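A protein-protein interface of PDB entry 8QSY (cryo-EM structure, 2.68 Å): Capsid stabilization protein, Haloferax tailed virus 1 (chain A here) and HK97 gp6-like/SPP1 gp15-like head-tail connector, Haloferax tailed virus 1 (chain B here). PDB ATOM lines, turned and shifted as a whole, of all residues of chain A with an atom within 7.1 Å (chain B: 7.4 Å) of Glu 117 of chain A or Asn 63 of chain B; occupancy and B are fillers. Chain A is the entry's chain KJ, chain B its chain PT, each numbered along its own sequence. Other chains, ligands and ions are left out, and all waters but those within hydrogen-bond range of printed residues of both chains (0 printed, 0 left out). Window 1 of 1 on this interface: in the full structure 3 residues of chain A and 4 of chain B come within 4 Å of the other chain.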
ATOM      1  N   VAL A  86     -11.848  15.294 -27.895  1.00  0.00           N
ATOM      2  CA  VAL A  86     -13.110  14.905 -28.525  1.00  0.00           C
ATOM      3  C   VAL A  86     -13.572  15.979 -29.512  1.00  0.00           C
ATOM      4  O   VAL A  86     -13.246  17.155 -29.380  1.00  0.00           O
ATOM      5  CB  VAL A  86     -14.226  14.619 -27.499  1.00  0.00           C
ATOM      6  CG1 VAL A  86     -13.836  13.553 -26.495  1.00  0.00           C
ATOM      7  CG2 VAL A  86     -14.698  15.874 -26.772  1.00  0.00           C
ATOM      8  N   THR A  87     -14.417  15.563 -30.461  1.00  0.00           N
ATOM      9  CA  THR A  87     -14.856  16.353 -31.603  1.00  0.00           C
ATOM     10  C   THR A  87     -16.367  16.202 -31.766  1.00  0.00           C
ATOM     11  O   THR A  87     -16.954  15.242 -31.275  1.00  0.00           O
ATOM     12  CB  THR A  87     -14.148  15.891 -32.886  1.00  0.00           C
ATOM     13  OG1 THR A  87     -14.489  14.535 -33.177  1.00  0.00           O
ATOM     14  CG2 THR A  87     -12.643  15.975 -32.799  1.00  0.00           C
ATOM     15  N   ALA A  88     -17.014  17.145 -32.462  1.00  0.00           N
ATOM     16  CA  ALA A  88     -18.445  17.029 -32.721  1.00  0.00           C
ATOM     17  C   ALA A  88     -18.773  15.696 -33.402  1.00  0.00           C
ATOM     18  O   ALA A  88     -17.995  15.206 -34.217  1.00  0.00           O
ATOM     19  CB  ALA A  88     -18.911  18.205 -33.538  1.00  0.00           C
ATOM     20  N   ASN A  89     -19.919  15.095 -33.034  1.00  0.00           N
ATOM     21  CA  ASN A  89     -20.364  13.774 -33.456  1.00  0.00           C
ATOM     22  C   ASN A  89     -19.672  12.603 -32.746  1.00  0.00           C
ATOM     23  O   ASN A  89     -20.112  11.468 -32.936  1.00  0.00           O
ATOM     24  CB  ASN A  89     -20.341  13.592 -34.978  1.00  0.00           C
ATOM     25  CG  ASN A  89     -21.376  12.607 -35.476  1.00  0.00           C
ATOM     26  OD1 ASN A  89     -22.574  12.817 -35.298  1.00  0.00           O
ATOM     27  ND2 ASN A  89     -20.930  11.525 -36.097  1.00  0.00           N
ATOM     28  N   ILE A 114     -23.583  12.450 -27.000  1.00  0.00           N
ATOM     29  CA  ILE A 114     -23.023  12.827 -28.285  1.00  0.00           C
ATOM     30  C   ILE A 114     -22.388  14.208 -28.131  1.00  0.00           C
ATOM     31  O   ILE A 114     -23.020  15.135 -27.637  1.00  0.00           O
ATOM     32  CB  ILE A 114     -24.109  12.751 -29.386  1.00  0.00           C
ATOM     33  CG1 ILE A 114     -23.543  12.980 -30.783  1.00  0.00           C
ATOM     34  CG2 ILE A 114     -25.291  13.673 -29.151  1.00  0.00           C
ATOM     35  CD1 ILE A 114     -22.966  11.744 -31.367  1.00  0.00           C
ATOM     36  N   VAL A 115     -21.114  14.334 -28.507  1.00  0.00           N
ATOM     37  CA  VAL A 115     -20.404  15.596 -28.383  1.00  0.00           C
ATOM     38  C   VAL A 115     -20.924  16.559 -29.446  1.00  0.00           C
ATOM     39  O   VAL A 115     -20.949  16.226 -30.626  1.00  0.00           O
ATOM     40  CB  VAL A 115     -18.889  15.367 -28.501  1.00  0.00           C
ATOM     41  CG1 VAL A 115     -18.117  16.672 -28.564  1.00  0.00           C
ATOM     42  CG2 VAL A 115     -18.395  14.531 -27.341  1.00  0.00           C
ATOM     43  N   GLN A 116     -21.312  17.764 -29.016  1.00  0.00           N
ATOM     44  CA  GLN A 116     -21.833  18.808 -29.889  1.00  0.00           C
ATOM     45  C   GLN A 116     -20.814  19.924 -30.114  1.00  0.00           C
ATOM     46  O   GLN A 116     -20.832  20.563 -31.163  1.00  0.00           O
ATOM     47  CB  GLN A 116     -23.106  19.396 -29.300  1.00  0.00           C
ATOM     48  CG  GLN A 116     -24.108  18.318 -28.963  1.00  0.00           C
ATOM     49  CD  GLN A 116     -25.503  18.872 -28.839  1.00  0.00           C
ATOM     50  OE1 GLN A 116     -26.380  18.559 -29.639  1.00  0.00           O
ATOM     51  NE2 GLN A 116     -25.728  19.713 -27.841  1.00  0.00           N
ATOM     52  N   GLU A 117     -19.935  20.154 -29.132  1.00  0.00           N
ATOM     53  CA  GLU A 117     -18.787  21.033 -29.292  1.00  0.00           C
ATOM     54  C   GLU A 117     -17.535  20.308 -28.794  1.00  0.00           C
ATOM     55  O   GLU A 117     -17.510  19.844 -27.662  1.00  0.00           O
ATOM     56  CB  GLU A 117     -19.046  22.335 -28.541  1.00  0.00           C
ATOM     57  CG  GLU A 117     -17.974  23.373 -28.779  1.00  0.00           C
ATOM     58  CD  GLU A 117     -17.950  24.476 -27.740  1.00  0.00           C
ATOM     59  OE1 GLU A 117     -18.839  25.351 -27.791  1.00  0.00           O
ATOM     60  OE2 GLU A 117     -17.049  24.459 -26.874  1.00  0.00           O
ATOM     61  N   GLY A 118     -16.500  20.219 -29.641  1.00  0.00           N
ATOM     62  CA  GLY A 118     -15.267  19.508 -29.308  1.00  0.00           C
ATOM     63  C   GLY A 118     -14.469  20.170 -28.179  1.00  0.00           C
ATOM     64  O   GLY A 118     -14.649  21.348 -27.875  1.00  0.00           O
ATOM     65  N   ALA A 119     -13.567  19.394 -27.561  1.00  0.00           N
ATOM     66  CA  ALA A 119     -12.741  19.856 -26.450  1.00  0.00           C
ATOM     67  C   ALA A 119     -11.427  19.067 -26.396  1.00  0.00           C
ATOM     68  O   ALA A 119     -11.384  17.907 -26.795  1.00  0.00           O
ATOM     69  CB  ALA A 119     -13.532  19.717 -25.168  1.00  0.00           C
ATOM     70  N   GLU A 123     -10.381  19.458 -20.789  1.00  0.00           N
ATOM     71  CA  GLU A 123     -11.345  20.538 -20.977  1.00  0.00           C
ATOM     72  C   GLU A 123     -12.785  20.038 -20.802  1.00  0.00           C
ATOM     73  O   GLU A 123     -13.051  18.844 -20.659  1.00  0.00           O
ATOM     74  CB  GLU A 123     -11.201  21.157 -22.368  1.00  0.00           C
ATOM     75  CG  GLU A 123      -9.929  21.946 -22.595  1.00  0.00           C
ATOM     76  CD  GLU A 123     -10.081  22.871 -23.788  1.00  0.00           C
ATOM     77  OE1 GLU A 123     -10.288  22.370 -24.922  1.00  0.00           O
ATOM     78  OE2 GLU A 123     -10.033  24.093 -23.576  1.00  0.00           O
ATOM     79  N   VAL A 124     -13.724  20.986 -20.863  1.00  0.00           N
ATOM     80  CA  VAL A 124     -15.152  20.711 -20.801  1.00  0.00           C
ATOM     81  C   VAL A 124     -15.732  20.806 -22.212  1.00  0.00           C
ATOM     82  O   VAL A 124     -15.616  21.838 -22.873  1.00  0.00           O
ATOM     83  CB  VAL A 124     -15.806  21.704 -19.821  1.00  0.00           C
ATOM     84  CG1 VAL A 124     -17.302  21.838 -20.003  1.00  0.00           C
ATOM     85  CG2 VAL A 124     -15.485  21.331 -18.390  1.00  0.00           C
ATOM     86  N   CYS A 125     -16.360  19.717 -22.679  1.00  0.00           N
ATOM     87  CA  CYS A 125     -17.103  19.713 -23.931  1.00  0.00           C
ATOM     88  C   CYS A 125     -18.579  20.031 -23.670  1.00  0.00           C
ATOM     89  O   CYS A 125     -19.038  20.010 -22.534  1.00  0.00           O
ATOM     90  CB  CYS A 125     -16.946  18.360 -24.617  1.00  0.00           C
ATOM     91  SG  CYS A 125     -17.941  17.068 -23.833  1.00  0.00           S
ATOM     92  N   GLU A 126     -19.332  20.321 -24.735  1.00  0.00           N
ATOM     93  CA  GLU A 126     -20.780  20.451 -24.654  1.00  0.00           C
ATOM     94  C   GLU A 126     -21.393  19.229 -25.335  1.00  0.00           C
ATOM     95  O   GLU A 126     -21.075  18.951 -26.488  1.00  0.00           O
ATOM     96  CB  GLU A 126     -21.215  21.785 -25.266  1.00  0.00           C
ATOM     97  CG  GLU A 126     -20.534  22.984 -24.616  1.00  0.00           C
ATOM     98  CD  GLU A 126     -21.277  24.314 -24.657  1.00  0.00           C
ATOM     99  OE1 GLU A 126     -22.070  24.523 -25.595  1.00  0.00           O
ATOM    100  OE2 GLU A 126     -21.082  25.141 -23.726  1.00  0.00           O
ATOM    101  N   ALA A 127     -22.264  18.497 -24.622  1.00  0.00           N
ATOM    102  CA  ALA A 127     -22.762  17.199 -25.073  1.00  0.00           C
ATOM    103  C   ALA A 127     -24.267  17.037 -24.822  1.00  0.00           C
ATOM    104  O   ALA A 127     -24.819  17.595 -23.877  1.00  0.00           O
ATOM    105  CB  ALA A 127     -21.971  16.103 -24.400  1.00  0.00           C
ATOM    106  N   TYR B  60      -3.792  27.938 -26.337  1.00  0.00           N
ATOM    107  CA  TYR B  60      -4.563  28.143 -27.559  1.00  0.00           C
ATOM    108  C   TYR B  60      -5.770  27.204 -27.621  1.00  0.00           C
ATOM    109  O   TYR B  60      -6.144  26.719 -28.692  1.00  0.00           O
ATOM    110  CB  TYR B  60      -3.633  28.044 -28.774  1.00  0.00           C
ATOM    111  CG  TYR B  60      -2.413  28.929 -28.680  1.00  0.00           C
ATOM    112  CD1 TYR B  60      -2.547  30.311 -28.678  1.00  0.00           C
ATOM    113  CD2 TYR B  60      -1.130  28.398 -28.583  1.00  0.00           C
ATOM    114  CE1 TYR B  60      -1.441  31.146 -28.589  1.00  0.00           C
ATOM    115  CE2 TYR B  60      -0.017  29.224 -28.484  1.00  0.00           C
ATOM    116  CZ  TYR B  60      -0.172  30.602 -28.485  1.00  0.00           C
ATOM    117  OH  TYR B  60       0.917  31.422 -28.372  1.00  0.00           O
ATOM    118  N   SER B  61      -6.380  26.963 -26.454  1.00  0.00           N
ATOM    119  CA  SER B  61      -7.568  26.138 -26.290  1.00  0.00           C
ATOM    120  C   SER B  61      -8.736  26.998 -25.789  1.00  0.00           C
ATOM    121  O   SER B  61      -8.676  28.226 -25.864  1.00  0.00           O
ATOM    122  CB  SER B  61      -7.252  24.968 -25.386  1.00  0.00           C
ATOM    123  OG  SER B  61      -6.877  25.434 -24.098  1.00  0.00           O
ATOM    124  N   GLY B  62      -9.833  26.361 -25.352  1.00  0.00           N
ATOM    125  CA  GLY B  62     -11.005  27.087 -24.878  1.00  0.00           C
ATOM    126  C   GLY B  62     -11.777  27.794 -25.992  1.00  0.00           C
ATOM    127  O   GLY B  62     -11.567  27.549 -27.178  1.00  0.00           O
ATOM    128  N   ASN B  63     -12.697  28.674 -25.581  1.00  0.00           N
ATOM    129  CA  ASN B  63     -13.611  29.349 -26.490  1.00  0.00           C
ATOM    130  C   ASN B  63     -13.556  30.860 -26.278  1.00  0.00           C
ATOM    131  O   ASN B  63     -13.098  31.355 -25.253  1.00  0.00           O
ATOM    132  CB  ASN B  63     -15.056  28.881 -26.305  1.00  0.00           C
ATOM    133  CG  ASN B  63     -15.219  27.377 -26.211  1.00  0.00           C
ATOM    134  OD1 ASN B  63     -15.324  26.828 -25.115  1.00  0.00           O
ATOM    135  ND2 ASN B  63     -15.298  26.705 -27.348  1.00  0.00           N
ATOM    136  N   MET B  64     -14.044  31.593 -27.271  1.00  0.00           N
ATOM    137  CA  MET B  64     -13.912  33.034 -27.311  1.00  0.00           C
ATOM    138  C   MET B  64     -15.155  33.598 -28.005  1.00  0.00           C
ATOM    139  O   MET B  64     -15.336  33.422 -29.215  1.00  0.00           O
ATOM    140  CB  MET B  64     -12.623  33.324 -28.081  1.00  0.00           C
ATOM    141  CG  MET B  64     -12.247  34.759 -28.105  1.00  0.00           C
ATOM    142  SD  MET B  64     -10.470  35.053 -28.190  1.00  0.00           S
ATOM    143  CE  MET B  64     -10.085  34.421 -29.827  1.00  0.00           C
ATOM    144  N   SER B  65     -16.076  34.181 -27.216  1.00  0.00           N
ATOM    145  CA  SER B  65     -17.429  34.509 -27.651  1.00  0.00           C
ATOM    146  C   SER B  65     -18.127  33.284 -28.265  1.00  0.00           C
ATOM    147  O   SER B  65     -18.805  33.375 -29.286  1.00  0.00           O
ATOM    148  CB  SER B  65     -17.432  35.723 -28.560  1.00  0.00           C
ATOM    149  OG  SER B  65     -18.743  36.012 -28.992  1.00  0.00           O
ATOM    150  N   ARG B  66     -17.951  32.124 -27.618  1.00  0.00           N
ATOM    151  CA  ARG B  66     -18.484  30.826 -28.018  1.00  0.00           C
ATOM    152  C   ARG B  66     -17.935  30.312 -29.361  1.00  0.00           C
ATOM    153  O   ARG B  66     -18.359  29.260 -29.831  1.00  0.00           O
ATOM    154  CB  ARG B  66     -20.008  30.835 -27.831  1.00  0.00           C
ATOM    155  CG  ARG B  66     -20.716  29.493 -27.930  1.00  0.00           C
ATOM    156  CD  ARG B  66     -20.090  28.318 -27.203  1.00  0.00           C
ATOM    157  NE  ARG B  66     -19.816  28.594 -25.804  1.00  0.00           N
ATOM    158  CZ  ARG B  66     -18.945  27.921 -25.067  1.00  0.00           C
ATOM    159  NH1 ARG B  66     -18.750  28.264 -23.808  1.00  0.00           N
ATOM    160  NH2 ARG B  66     -18.286  26.891 -25.572  1.00  0.00           N
ATOM    161  N   LEU B  67     -16.967  31.014 -29.971  1.00  0.00           N
ATOM    162  CA  LEU B  67     -16.188  30.533 -31.111  1.00  0.00           C
ATOM    163  C   LEU B  67     -14.997  29.724 -30.603  1.00  0.00           C
ATOM    164  O   LEU B  67     -14.507  29.992 -29.515  1.00  0.00           O
ATOM    165  CB  LEU B  67     -15.685  31.733 -31.929  1.00  0.00           C
ATOM    166  CG  LEU B  67     -16.742  32.791 -32.250  1.00  0.00           C
ATOM    167  CD1 LEU B  67     -16.135  34.065 -32.814  1.00  0.00           C
ATOM    168  CD2 LEU B  67     -17.779  32.232 -33.212  1.00  0.00           C
ATOM    169  N   PRO B  68     -14.444  28.762 -31.372  1.00  0.00           N
ATOM    170  CA  PRO B  68     -13.181  28.132 -30.989  1.00  0.00           C
ATOM    171  C   PRO B  68     -12.044  29.153 -31.066  1.00  0.00           C
ATOM    172  O   PRO B  68     -12.035  30.007 -31.954  1.00  0.00           O
ATOM    173  CB  PRO B  68     -12.985  27.039 -32.047  1.00  0.00           C
ATOM    174  CG  PRO B  68     -13.745  27.554 -33.250  1.00  0.00           C
ATOM    175  CD  PRO B  68     -14.933  28.292 -32.673  1.00  0.00           C
ATOM    176  N   THR B  69     -11.073  29.070 -30.149  1.00  0.00           N
ATOM    177  CA  THR B  69      -9.871  29.889 -30.260  1.00  0.00           C
ATOM    178  C   THR B  69      -8.991  29.392 -31.402  1.00  0.00           C
ATOM    179  O   THR B  69      -8.536  30.194 -32.206  1.00  0.00           O
ATOM    180  CB  THR B  69      -9.042  29.920 -28.976  1.00  0.00           C
ATOM    181  OG1 THR B  69      -8.846  28.572 -28.561  1.00  0.00           O
ATOM    182  CG2 THR B  69      -9.737  30.664 -27.864  1.00  0.00           C
ATOM    183  N   LEU B  70      -8.789  28.073 -31.495  1.00  0.00           N
ATOM    184  CA  LEU B  70      -8.101  27.472 -32.620  1.00  0.00           C
ATOM    185  C   LEU B  70      -9.113  27.277 -33.752  1.00  0.00           C
ATOM    186  O   LEU B  70      -9.717  26.212 -33.903  1.00  0.00           O
ATOM    187  CB  LEU B  70      -7.437  26.186 -32.122  1.00  0.00           C
ATOM    188  CG  LEU B  70      -6.702  25.330 -33.149  1.00  0.00           C
ATOM    189  CD1 LEU B  70      -5.832  26.152 -34.074  1.00  0.00           C
ATOM    190  CD2 LEU B  70      -5.840  24.317 -32.444  1.00  0.00           C
ATOM    191  N   ALA B 136     -13.488  37.724 -27.103  1.00  0.00           N
ATOM    192  CA  ALA B 136     -14.350  37.069 -26.119  1.00  0.00           C
ATOM    193  C   ALA B 136     -15.473  37.999 -25.663  1.00  0.00           C
ATOM    194  O   ALA B 136     -15.268  39.199 -25.500  1.00  0.00           O
ATOM    195  CB  ALA B 136     -13.536  36.607 -24.940  1.00  0.00           C
ATOM    196  N   ALA B 137     -16.660  37.428 -25.433  1.00  0.00           N
ATOM    197  CA  ALA B 137     -17.821  38.173 -24.971  1.00  0.00           C
ATOM    198  C   ALA B 137     -18.713  37.260 -24.138  1.00  0.00           C
ATOM    199  O   ALA B 137     -18.863  36.077 -24.440  1.00  0.00           O
ATOM    200  CB  ALA B 137     -18.582  38.758 -26.137  1.00  0.00           C
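The side-chain carboxylate of Glu 117 of chain A sits at hydrogen-bond distance from the side-chain amide nitrogen of Asn 63 of chain B, 2.9 Å away.
OE1 of Glu 117 of chain A is in salt-bridge range of NH2 of Arg 66 of chain B (2.8 Å).
The side-chain carboxylate of Glu 123 of chain A lies close to the side-chain hydroxyl of Ser 61 of chain B (3.5 Å).
The side-chain carboxylate (OE2) of Glu 123 of chain A is in hydrogen-bond range of the backbone NH (N) of Gly 62 of chain B.
The side-chain carboxylate of Glu 126 of chain A is in salt-bridge range of the guanidinium group of Arg 66 of chain B (3.8 Å).
The backbone NH (N) of Gln 116 of chain A sits at hydrogen-bond distance from the backbone carbonyl oxygen (O) of Glu 126 of chain A (2.8 Å).
O of Glu 126 of chain A sits at hydrogen-bond distance from N of Glu 117 of chain A (3.1 Å).
O of Ser 61 of chain B is in hydrogen-bond range of OG1 of Thr 69 of chain B, at 2.7 Å.
The side-chain hydroxyl (OG1) of Thr 69 of chain B is in hydrogen-bond range of the backbone carbonyl oxygen (O) of Gly 62 of chain B, at 3.2 Å.
The side-chain amide oxygen of Asn 63 of chain B lies within hydrogen-bond range of the guanidinium group of Arg 66 of chain B (3.0 Å).
No residue of chain B comes within 4 Å of Gly 118 of chain A.
Of the printed residues of chain B, Glu 126 of chain A touches Arg 66.
Of the printed residues of chain A, Gly 62 of chain B touches Glu 123 (2.9 Å).
Of the printed residues of chain A, Arg 66 of chain B touches Glu 117 (2.8 Å) and Glu 126 (3.8 Å).
Of the printed residues of chain B, Glu 123 of chain A touches Ser 61 and Gly 62.
Ala 137 of chain B touches none of the printed residues of chain A.
The nearest residue of chain A that does not touch Asn 63 of chain B is Gly 118 of chain A (5.4 Å).
Printed residues of chain B that touch a printed residue of chain A: Ser 61, Gly 62, Asn 63 and Arg 66.
Among the printed residues, 5 pairs touch across the chains.
Among the printed residues, Asp or Glu carboxylates within 4 Å of a Lys or Arg side-chain nitrogen of the other chain: Glu 117 of chain A with Arg 66 of chain B and Glu 126 of chain A with Arg 66 of chain B.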
